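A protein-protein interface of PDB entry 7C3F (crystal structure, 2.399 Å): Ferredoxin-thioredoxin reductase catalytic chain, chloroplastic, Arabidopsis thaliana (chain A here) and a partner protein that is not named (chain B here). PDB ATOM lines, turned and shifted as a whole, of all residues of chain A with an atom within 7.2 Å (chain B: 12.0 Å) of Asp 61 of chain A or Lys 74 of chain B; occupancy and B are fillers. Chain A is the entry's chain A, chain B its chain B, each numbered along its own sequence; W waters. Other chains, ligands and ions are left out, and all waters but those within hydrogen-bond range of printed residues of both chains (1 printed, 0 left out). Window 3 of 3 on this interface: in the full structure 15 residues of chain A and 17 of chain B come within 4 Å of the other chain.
Among the printed residues, pairs that only touch across the chains: Glu 65 of chain A with Ile 76 of chain B (3.3 Å), Ala 64 of chain A with Ile 76 of chain B (3.3 Å), Gly 67 of chain A with Trp 71 of chain B (3.5 Å), Ala 64 of chain A with Trp 71 of chain B (3.6 Å), Asp 61 of chain A with Lys 74 of chain B (3.7 Å), Tyr 59 of chain A with Ser 77 of chain B (3.8 Å) and Ala 64 of chain A with Lys 74 of chain B (3.9 Å).
Water W1 bridges OD2 of Asp 61 of chain A and N of Lys 75 of chain B.
The side-chain carboxylate of Asp 61 of chain A sits at hydrogen-bond distance from the backbone NH of Ala 64 of chain A (3.4 Å). O of Val 69 of chain B is in hydrogen-bond range of N of Ile 76 of chain B (2.7 Å).
The side-chain hydroxyl (OG) of Ser 77 of chain B lies within hydrogen-bond range of the side-chain carboxylate (OE1) of Glu 65 of chain A, at 2.6 Å.
Of the 19 printed residues of chain B, 4 touch a printed residue of chain A. Printed residues of chain B that touch a printed residue of chain A: Trp 71, Lys 74, Ile 76 and Ser 77. Hydrophobic or aromatic side chains of chain B that line the printed part of chain A: Trp 71 and Ile 76. Of the 11 printed residues of chain A, 5 touch a printed residue of chain B. Printed residues of chain A that touch a printed residue of chain B: Tyr 59, Asp 61, Ala 64, Glu 65 and Gly 67. Hydrophobic or aromatic side chains of chain A that line the printed part of chain B: Tyr 59 and Ala 64. Among the printed residues, no Asp or Glu carboxylate lies within 4 Å of a Lys or Arg side-chain nitrogen of the other chain.
Of the printed residues of chain B, Tyr 59 of chain A touches Ser 77 (3.8 Å). No residue of chain B comes within 4 Å of Lys 62 of chain A. No residue of chain B comes within 4 Å of Ala 63 of chain A. Of the printed residues of chain B, Gly 67 of chain A touches Trp 71. Glu 28 of chain B touches none of the printed residues of chain A. Printed residues of chain A within 4 Å of Trp 71 of chain B: Ala 64 (3.6 Å) and Gly 67 (3.5 Å). No residue of chain A comes within 4 Å of Gly 73 of chain B. Of the printed residues of chain A, Lys 74 of chain B touches Asp 61 (3.7 Å) and Ala 64 (3.9 Å). Printed residues of chain A within 4 Å of Ile 76 of chain B: Ala 64 (3.3 Å) and Glu 65 (3.3 Å). Of the printed residues of chain A, Ser 77 of chain B touches Tyr 59 and Glu 65. The nearest printed residue of chain A that does not touch Ser 77 of chain B is His 58 of chain A (4.4 Å).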
ATOM      1  N   LEU A  53     -33.934 -21.234  25.089  1.00  0.00           N
ATOM      2  CA  LEU A  53     -33.414 -21.320  23.733  1.00  0.00           C
ATOM      3  C   LEU A  53     -34.062 -22.486  22.996  1.00  0.00           C
ATOM      4  O   LEU A  53     -34.405 -23.507  23.595  1.00  0.00           O
ATOM      5  CB  LEU A  53     -31.895 -21.508  23.758  1.00  0.00           C
ATOM      6  CG  LEU A  53     -30.959 -20.367  23.370  1.00  0.00           C
ATOM      7  CD1 LEU A  53     -29.536 -20.897  23.215  1.00  0.00           C
ATOM      8  CD2 LEU A  53     -31.421 -19.664  22.097  1.00  0.00           C
ATOM      9  N   HIS A  58     -29.003 -25.918  16.338  1.00  0.00           N
ATOM     10  CA  HIS A  58     -27.625 -26.051  16.788  1.00  0.00           C
ATOM     11  C   HIS A  58     -26.965 -24.679  16.772  1.00  0.00           C
ATOM     12  O   HIS A  58     -27.039 -23.962  15.768  1.00  0.00           O
ATOM     13  CB  HIS A  58     -26.843 -27.029  15.910  1.00  0.00           C
ATOM     14  CG  HIS A  58     -25.379 -27.058  16.208  1.00  0.00           C
ATOM     15  ND1 HIS A  58     -24.857 -27.704  17.308  1.00  0.00           N
ATOM     16  CD2 HIS A  58     -24.326 -26.504  15.562  1.00  0.00           C
ATOM     17  CE1 HIS A  58     -23.545 -27.553  17.323  1.00  0.00           C
ATOM     18  NE2 HIS A  58     -23.197 -26.828  16.275  1.00  0.00           N
ATOM     19  N   TYR A  59     -26.333 -24.313  17.882  1.00  0.00           N
ATOM     20  CA  TYR A  59     -25.728 -23.000  18.023  1.00  0.00           C
ATOM     21  C   TYR A  59     -24.215 -23.111  18.145  1.00  0.00           C
ATOM     22  O   TYR A  59     -23.681 -24.115  18.626  1.00  0.00           O
ATOM     23  CB  TYR A  59     -26.278 -22.265  19.247  1.00  0.00           C
ATOM     24  CG  TYR A  59     -27.782 -22.317  19.378  1.00  0.00           C
ATOM     25  CD1 TYR A  59     -28.588 -21.418  18.693  1.00  0.00           C
ATOM     26  CD2 TYR A  59     -28.394 -23.257  20.194  1.00  0.00           C
ATOM     27  CE1 TYR A  59     -29.965 -21.456  18.815  1.00  0.00           C
ATOM     28  CE2 TYR A  59     -29.769 -23.305  20.321  1.00  0.00           C
ATOM     29  CZ  TYR A  59     -30.549 -22.403  19.631  1.00  0.00           C
ATOM     30  OH  TYR A  59     -31.917 -22.448  19.755  1.00  0.00           O
ATOM     31  N   ASP A  60     -23.532 -22.051  17.715  1.00  0.00           N
ATOM     32  CA  ASP A  60     -22.107 -21.893  17.960  1.00  0.00           C
ATOM     33  C   ASP A  60     -21.837 -21.164  19.264  1.00  0.00           C
ATOM     34  O   ASP A  60     -20.841 -21.453  19.936  1.00  0.00           O
ATOM     35  CB  ASP A  60     -21.445 -21.114  16.819  1.00  0.00           C
ATOM     36  CG  ASP A  60     -21.385 -21.901  15.523  1.00  0.00           C
ATOM     37  OD1 ASP A  60     -21.426 -23.149  15.571  1.00  0.00           O
ATOM     38  OD2 ASP A  60     -21.286 -21.264  14.454  1.00  0.00           O
ATOM     39  N   ASP A  61     -22.717 -20.233  19.637  1.00  0.00           N
ATOM     40  CA  ASP A  61     -22.519 -19.346  20.785  1.00  0.00           C
ATOM     41  C   ASP A  61     -23.867 -19.204  21.490  1.00  0.00           C
ATOM     42  O   ASP A  61     -24.619 -18.263  21.225  1.00  0.00           O
ATOM     43  CB  ASP A  61     -21.972 -18.001  20.318  1.00  0.00           C
ATOM     44  CG  ASP A  61     -21.438 -17.155  21.455  1.00  0.00           C
ATOM     45  OD1 ASP A  61     -21.648 -17.523  22.629  1.00  0.00           O
ATOM     46  OD2 ASP A  61     -20.809 -16.115  21.167  1.00  0.00           O
ATOM     47  N   LYS A  62     -24.157 -20.137  22.402  1.00  0.00           N
ATOM     48  CA  LYS A  62     -25.463 -20.155  23.056  1.00  0.00           C
ATOM     49  C   LYS A  62     -25.674 -18.922  23.929  1.00  0.00           C
ATOM     50  O   LYS A  62     -26.797 -18.413  24.029  1.00  0.00           O
ATOM     51  CB  LYS A  62     -25.624 -21.441  23.868  1.00  0.00           C
ATOM     52  CG  LYS A  62     -25.726 -22.678  22.988  1.00  0.00           C
ATOM     53  CD  LYS A  62     -25.670 -23.967  23.788  1.00  0.00           C
ATOM     54  CE  LYS A  62     -27.058 -24.547  23.991  1.00  0.00           C
ATOM     55  NZ  LYS A  62     -27.090 -26.016  23.747  1.00  0.00           N
ATOM     56  N   ALA A  63     -24.617 -18.438  24.584  1.00  0.00           N
ATOM     57  CA  ALA A  63     -24.747 -17.232  25.398  1.00  0.00           C
ATOM     58  C   ALA A  63     -25.115 -16.027  24.544  1.00  0.00           C
ATOM     59  O   ALA A  63     -25.966 -15.217  24.932  1.00  0.00           O
ATOM     60  CB  ALA A  63     -23.451 -16.971  26.164  1.00  0.00           C
ATOM     61  N   ALA A  64     -24.482 -15.889  23.378  1.00  0.00           N
ATOM     62  CA  ALA A  64     -24.821 -14.789  22.481  1.00  0.00           C
ATOM     63  C   ALA A  64     -26.243 -14.926  21.950  1.00  0.00           C
ATOM     64  O   ALA A  64     -26.954 -13.925  21.805  1.00  0.00           O
ATOM     65  CB  ALA A  64     -23.822 -14.720  21.327  1.00  0.00           C
ATOM     66  N   GLU A  65     -26.664 -16.153  21.631  1.00  0.00           N
ATOM     67  CA  GLU A  65     -28.025 -16.370  21.151  1.00  0.00           C
ATOM     68  C   GLU A  65     -29.046 -15.929  22.191  1.00  0.00           C
ATOM     69  O   GLU A  65     -30.036 -15.262  21.866  1.00  0.00           O
ATOM     70  CB  GLU A  65     -28.227 -17.841  20.785  1.00  0.00           C
ATOM     71  CG  GLU A  65     -27.349 -18.329  19.648  1.00  0.00           C
ATOM     72  CD  GLU A  65     -27.929 -18.014  18.287  1.00  0.00           C
ATOM     73  OE1 GLU A  65     -27.289 -18.363  17.272  1.00  0.00           O
ATOM     74  OE2 GLU A  65     -29.024 -17.417  18.234  1.00  0.00           O
ATOM     75  N   VAL A  66     -28.819 -16.298  23.454  1.00  0.00           N
ATOM     76  CA  VAL A  66     -29.711 -15.874  24.530  1.00  0.00           C
ATOM     77  C   VAL A  66     -29.724 -14.355  24.642  1.00  0.00           C
ATOM     78  O   VAL A  66     -30.775 -13.740  24.872  1.00  0.00           O
ATOM     79  CB  VAL A  66     -29.295 -16.542  25.854  1.00  0.00           C
ATOM     80  CG1 VAL A  66     -29.849 -15.775  27.051  1.00  0.00           C
ATOM     81  CG2 VAL A  66     -29.758 -17.989  25.883  1.00  0.00           C
ATOM     82  N   GLY A  67     -28.563 -13.724  24.461  1.00  0.00           N
ATOM     83  CA  GLY A  67     -28.492 -12.277  24.589  1.00  0.00           C
ATOM     84  C   GLY A  67     -29.235 -11.555  23.480  1.00  0.00           C
ATOM     85  O   GLY A  67     -29.988 -10.612  23.736  1.00  0.00           O
ATOM     86  N   THR B  24     -16.605 -13.672   6.041  1.00  0.00           N
ATOM     87  CA  THR B  24     -17.218 -12.412   6.419  1.00  0.00           C
ATOM     88  C   THR B  24     -17.492 -11.577   5.183  1.00  0.00           C
ATOM     89  O   THR B  24     -17.801 -10.381   5.275  1.00  0.00           O
ATOM     90  CB  THR B  24     -16.322 -11.630   7.396  1.00  0.00           C
ATOM     91  OG1 THR B  24     -17.118 -10.753   8.207  1.00  0.00           O
ATOM     92  CG2 THR B  24     -15.238 -10.829   6.645  1.00  0.00           C
ATOM     93  N   ASP B  27     -21.191 -11.404   5.150  1.00  0.00           N
ATOM     94  CA  ASP B  27     -21.611 -10.511   6.218  1.00  0.00           C
ATOM     95  C   ASP B  27     -21.295  -9.053   5.874  1.00  0.00           C
ATOM     96  O   ASP B  27     -22.071  -8.152   6.225  1.00  0.00           O
ATOM     97  CB  ASP B  27     -20.975 -10.968   7.537  1.00  0.00           C
ATOM     98  CG  ASP B  27     -21.556 -12.313   8.033  1.00  0.00           C
ATOM     99  OD1 ASP B  27     -22.643 -12.680   7.543  1.00  0.00           O
ATOM    100  OD2 ASP B  27     -20.951 -13.007   8.888  1.00  0.00           O
ATOM    101  N   GLU B  28     -20.189  -8.803   5.155  1.00  0.00           N
ATOM    102  CA  GLU B  28     -19.843  -7.432   4.779  1.00  0.00           C
ATOM    103  C   GLU B  28     -20.726  -6.933   3.641  1.00  0.00           C
ATOM    104  O   GLU B  28     -21.094  -5.753   3.602  1.00  0.00           O
ATOM    105  CB  GLU B  28     -18.365  -7.343   4.394  1.00  0.00           C
ATOM    106  CG  GLU B  28     -17.671  -6.083   4.880  1.00  0.00           C
ATOM    107  CD  GLU B  28     -17.570  -6.017   6.398  1.00  0.00           C
ATOM    108  OE1 GLU B  28     -17.793  -4.927   6.967  1.00  0.00           O
ATOM    109  OE2 GLU B  28     -17.265  -7.056   7.024  1.00  0.00           O
ATOM    110  N   LYS B  31     -24.050  -6.176   5.502  1.00  0.00           N
ATOM    111  CA  LYS B  31     -23.970  -4.964   6.292  1.00  0.00           C
ATOM    112  C   LYS B  31     -24.141  -3.725   5.429  1.00  0.00           C
ATOM    113  O   LYS B  31     -24.674  -2.718   5.901  1.00  0.00           O
ATOM    114  CB  LYS B  31     -22.644  -4.920   7.045  1.00  0.00           C
ATOM    115  CG  LYS B  31     -22.754  -4.249   8.405  1.00  0.00           C
ATOM    116  CD  LYS B  31     -21.603  -4.652   9.307  1.00  0.00           C
ATOM    117  CE  LYS B  31     -20.278  -4.154   8.762  1.00  0.00           C
ATOM    118  NZ  LYS B  31     -19.203  -4.188   9.793  1.00  0.00           N
ATOM    119  N   ILE B  34     -27.718  -2.241   5.118  1.00  0.00           N
ATOM    120  CA  ILE B  34     -28.393  -1.600   6.243  1.00  0.00           C
ATOM    121  C   ILE B  34     -28.749  -0.169   5.870  1.00  0.00           C
ATOM    122  O   ILE B  34     -27.920   0.579   5.339  1.00  0.00           O
ATOM    123  CB  ILE B  34     -27.509  -1.650   7.498  1.00  0.00           C
ATOM    124  CG1 ILE B  34     -27.191  -3.098   7.874  1.00  0.00           C
ATOM    125  CG2 ILE B  34     -28.191  -0.939   8.656  1.00  0.00           C
ATOM    126  CD1 ILE B  34     -26.440  -3.240   9.185  1.00  0.00           C
ATOM    127  N   ASP B  66     -31.374  -3.172  10.492  1.00  0.00           N
ATOM    128  CA  ASP B  66     -30.276  -3.920  11.090  1.00  0.00           C
ATOM    129  C   ASP B  66     -30.094  -5.250  10.381  1.00  0.00           C
ATOM    130  O   ASP B  66     -31.036  -5.804   9.809  1.00  0.00           O
ATOM    131  CB  ASP B  66     -30.508  -4.166  12.586  1.00  0.00           C
ATOM    132  CG  ASP B  66     -29.243  -4.589  13.305  1.00  0.00           C
ATOM    133  OD1 ASP B  66     -28.163  -4.563  12.671  1.00  0.00           O
ATOM    134  OD2 ASP B  66     -29.323  -4.948  14.497  1.00  0.00           O
ATOM    135  N   TYR B  67     -28.862  -5.748  10.443  1.00  0.00           N
ATOM    136  CA  TYR B  67     -28.497  -7.103  10.048  1.00  0.00           C
ATOM    137  C   TYR B  67     -28.217  -7.849  11.349  1.00  0.00           C
ATOM    138  O   TYR B  67     -27.109  -7.783  11.887  1.00  0.00           O
ATOM    139  CB  TYR B  67     -27.284  -7.090   9.121  1.00  0.00           C
ATOM    140  CG  TYR B  67     -26.829  -8.449   8.641  1.00  0.00           C
ATOM    141  CD1 TYR B  67     -27.684  -9.282   7.932  1.00  0.00           C
ATOM    142  CD2 TYR B  67     -25.534  -8.892   8.882  1.00  0.00           C
ATOM    143  CE1 TYR B  67     -27.266 -10.522   7.485  1.00  0.00           C
ATOM    144  CE2 TYR B  67     -25.108 -10.131   8.439  1.00  0.00           C
ATOM    145  CZ  TYR B  67     -25.978 -10.941   7.741  1.00  0.00           C
ATOM    146  OH  TYR B  67     -25.560 -12.174   7.297  1.00  0.00           O
ATOM    147  N   VAL B  68     -29.235  -8.548  11.865  1.00  0.00           N
ATOM    148  CA  VAL B  68     -29.189  -9.040  13.242  1.00  0.00           C
ATOM    149  C   VAL B  68     -28.292 -10.253  13.417  1.00  0.00           C
ATOM    150  O   VAL B  68     -28.145 -10.739  14.546  1.00  0.00           O
ATOM    151  CB  VAL B  68     -30.606  -9.386  13.741  1.00  0.00           C
ATOM    152  CG1 VAL B  68     -31.565  -8.236  13.460  1.00  0.00           C
ATOM    153  CG2 VAL B  68     -31.101 -10.668  13.096  1.00  0.00           C
ATOM    154  N   VAL B  69     -27.673 -10.748  12.344  1.00  0.00           N
ATOM    155  CA  VAL B  69     -26.671 -11.801  12.484  1.00  0.00           C
ATOM    156  C   VAL B  69     -25.495 -11.309  13.317  1.00  0.00           C
ATOM    157  O   VAL B  69     -24.908 -12.072  14.094  1.00  0.00           O
ATOM    158  CB  VAL B  69     -26.225 -12.293  11.092  1.00  0.00           C
ATOM    159  CG1 VAL B  69     -24.820 -12.871  11.141  1.00  0.00           C
ATOM    160  CG2 VAL B  69     -27.210 -13.324  10.563  1.00  0.00           C
ATOM    161  N   LEU B  70     -25.157 -10.029  13.204  1.00  0.00           N
ATOM    162  CA  LEU B  70     -24.072  -9.442  13.976  1.00  0.00           C
ATOM    163  C   LEU B  70     -24.663  -8.731  15.185  1.00  0.00           C
ATOM    164  O   LEU B  70     -25.565  -7.901  15.043  1.00  0.00           O
ATOM    165  CB  LEU B  70     -23.262  -8.465  13.124  1.00  0.00           C
ATOM    166  CG  LEU B  70     -22.850  -8.992  11.747  1.00  0.00           C
ATOM    167  CD1 LEU B  70     -21.990  -7.978  11.008  1.00  0.00           C
ATOM    168  CD2 LEU B  70     -22.127 -10.328  11.867  1.00  0.00           C
ATOM    169  N   TRP B  71     -24.146  -9.052  16.368  1.00  0.00           N
ATOM    170  CA  TRP B  71     -24.710  -8.538  17.612  1.00  0.00           C
ATOM    171  C   TRP B  71     -23.579  -8.395  18.620  1.00  0.00           C
ATOM    172  O   TRP B  71     -23.078  -9.403  19.128  1.00  0.00           O
ATOM    173  CB  TRP B  71     -25.803  -9.460  18.143  1.00  0.00           C
ATOM    174  CG  TRP B  71     -26.355  -9.024  19.461  1.00  0.00           C
ATOM    175  CD1 TRP B  71     -27.259  -8.024  19.678  1.00  0.00           C
ATOM    176  CD2 TRP B  71     -26.046  -9.574  20.749  1.00  0.00           C
ATOM    177  NE1 TRP B  71     -27.530  -7.917  21.020  1.00  0.00           N
ATOM    178  CE2 TRP B  71     -26.799  -8.854  21.700  1.00  0.00           C
ATOM    179  CE3 TRP B  71     -25.206 -10.601  21.189  1.00  0.00           C
ATOM    180  CZ2 TRP B  71     -26.738  -9.130  23.064  1.00  0.00           C
ATOM    181  CZ3 TRP B  71     -25.145 -10.872  22.546  1.00  0.00           C
ATOM    182  CH2 TRP B  71     -25.907 -10.140  23.467  1.00  0.00           C
ATOM    183  N   LYS B  72     -23.194  -7.152  18.908  1.00  0.00           N
ATOM    184  CA  LYS B  72     -22.195  -6.843  19.931  1.00  0.00           C
ATOM    185  C   LYS B  72     -20.907  -7.634  19.705  1.00  0.00           C
ATOM    186  O   LYS B  72     -20.341  -8.233  20.621  1.00  0.00           O
ATOM    187  CB  LYS B  72     -22.762  -7.094  21.330  1.00  0.00           C
ATOM    188  CG  LYS B  72     -24.047  -6.331  21.607  1.00  0.00           C
ATOM    189  CD  LYS B  72     -24.406  -6.337  23.085  1.00  0.00           C
ATOM    190  CE  LYS B  72     -25.616  -5.454  23.359  1.00  0.00           C
ATOM    191  NZ  LYS B  72     -26.011  -5.475  24.795  1.00  0.00           N
ATOM    192  N   GLY B  73     -20.451  -7.641  18.452  1.00  0.00           N
ATOM    193  CA  GLY B  73     -19.232  -8.327  18.077  1.00  0.00           C
ATOM    194  C   GLY B  73     -19.350  -9.823  17.888  1.00  0.00           C
ATOM    195  O   GLY B  73     -18.411 -10.439  17.365  1.00  0.00           O
ATOM    196  N   LYS B  74     -20.461 -10.427  18.290  1.00  0.00           N
ATOM    197  CA  LYS B  74     -20.677 -11.860  18.165  1.00  0.00           C
ATOM    198  C   LYS B  74     -21.626 -12.157  17.008  1.00  0.00           C
ATOM    199  O   LYS B  74     -22.279 -11.265  16.461  1.00  0.00           O
ATOM    200  CB  LYS B  74     -21.213 -12.430  19.482  1.00  0.00           C
ATOM    201  CG  LYS B  74     -20.142 -12.559  20.554  1.00  0.00           C
ATOM    202  CD  LYS B  74     -20.702 -12.283  21.940  1.00  0.00           C
ATOM    203  CE  LYS B  74     -19.860 -12.949  23.018  1.00  0.00           C
ATOM    204  NZ  LYS B  74     -18.405 -12.714  22.812  1.00  0.00           N
ATOM    205  N   LYS B  75     -21.692 -13.431  16.628  1.00  0.00           N
ATOM    206  CA  LYS B  75     -22.500 -13.870  15.499  1.00  0.00           C
ATOM    207  C   LYS B  75     -23.659 -14.735  15.973  1.00  0.00           C
ATOM    208  O   LYS B  75     -23.492 -15.601  16.838  1.00  0.00           O
ATOM    209  CB  LYS B  75     -21.662 -14.654  14.484  1.00  0.00           C
ATOM    210  CG  LYS B  75     -21.052 -13.794  13.389  1.00  0.00           C
ATOM    211  CD  LYS B  75     -20.675 -14.618  12.164  1.00  0.00           C
ATOM    212  CE  LYS B  75     -21.892 -15.269  11.524  1.00  0.00           C
ATOM    213  NZ  LYS B  75     -21.651 -15.587  10.087  1.00  0.00           N
ATOM    214  N   ILE B  76     -24.832 -14.487  15.394  1.00  0.00           N
ATOM    215  CA  ILE B  76     -26.079 -15.135  15.773  1.00  0.00           C
ATOM    216  C   ILE B  76     -26.571 -15.918  14.565  1.00  0.00           C
ATOM    217  O   ILE B  76     -26.410 -15.473  13.424  1.00  0.00           O
ATOM    218  CB  ILE B  76     -27.127 -14.098  16.237  1.00  0.00           C
ATOM    219  CG1 ILE B  76     -26.650 -13.401  17.510  1.00  0.00           C
ATOM    220  CG2 ILE B  76     -28.483 -14.739  16.473  1.00  0.00           C
ATOM    221  CD1 ILE B  76     -26.268 -14.358  18.609  1.00  0.00           C
ATOM    222  N   SER B  77     -27.168 -17.082  14.814  1.00  0.00           N
ATOM    223  CA  SER B  77     -27.641 -17.948  13.733  1.00  0.00           C
ATOM    224  C   SER B  77     -29.114 -17.681  13.421  1.00  0.00           C
ATOM    225  O   SER B  77     -29.966 -18.567  13.482  1.00  0.00           O
ATOM    226  CB  SER B  77     -27.409 -19.410  14.095  1.00  0.00           C
ATOM    227  OG  SER B  77     -28.157 -19.772  15.244  1.00  0.00           O
ATOM    228  N   ALA B  78     -29.406 -16.437  13.057  1.00  0.00           N
ATOM    229  CA  ALA B  78     -30.775 -16.055  12.750  1.00  0.00           C
ATOM    230  C   ALA B  78     -31.087 -16.387  11.296  1.00  0.00           C
ATOM    231  O   ALA B  78     -30.335 -16.013  10.391  1.00  0.00           O
ATOM    232  CB  ALA B  78     -30.988 -14.566  13.016  1.00  0.00           C
ATOM    233  N   PRO B  81     -32.402 -12.715   8.856  1.00  0.00           N
ATOM    234  CA  PRO B  81     -31.387 -11.825   9.441  1.00  0.00           C
ATOM    235  C   PRO B  81     -31.664 -10.334   9.310  1.00  0.00           C
ATOM    236  O   PRO B  81     -31.057  -9.554  10.057  1.00  0.00           O
ATOM    237  CB  PRO B  81     -30.115 -12.208   8.677  1.00  0.00           C
ATOM    238  CG  PRO B  81     -30.612 -12.661   7.344  1.00  0.00           C
ATOM    239  CD  PRO B  81     -31.966 -13.292   7.572  1.00  0.00           C
HETATM  240  O   HOH W   1     -20.251 -15.425  18.411  1.00  0.00           O
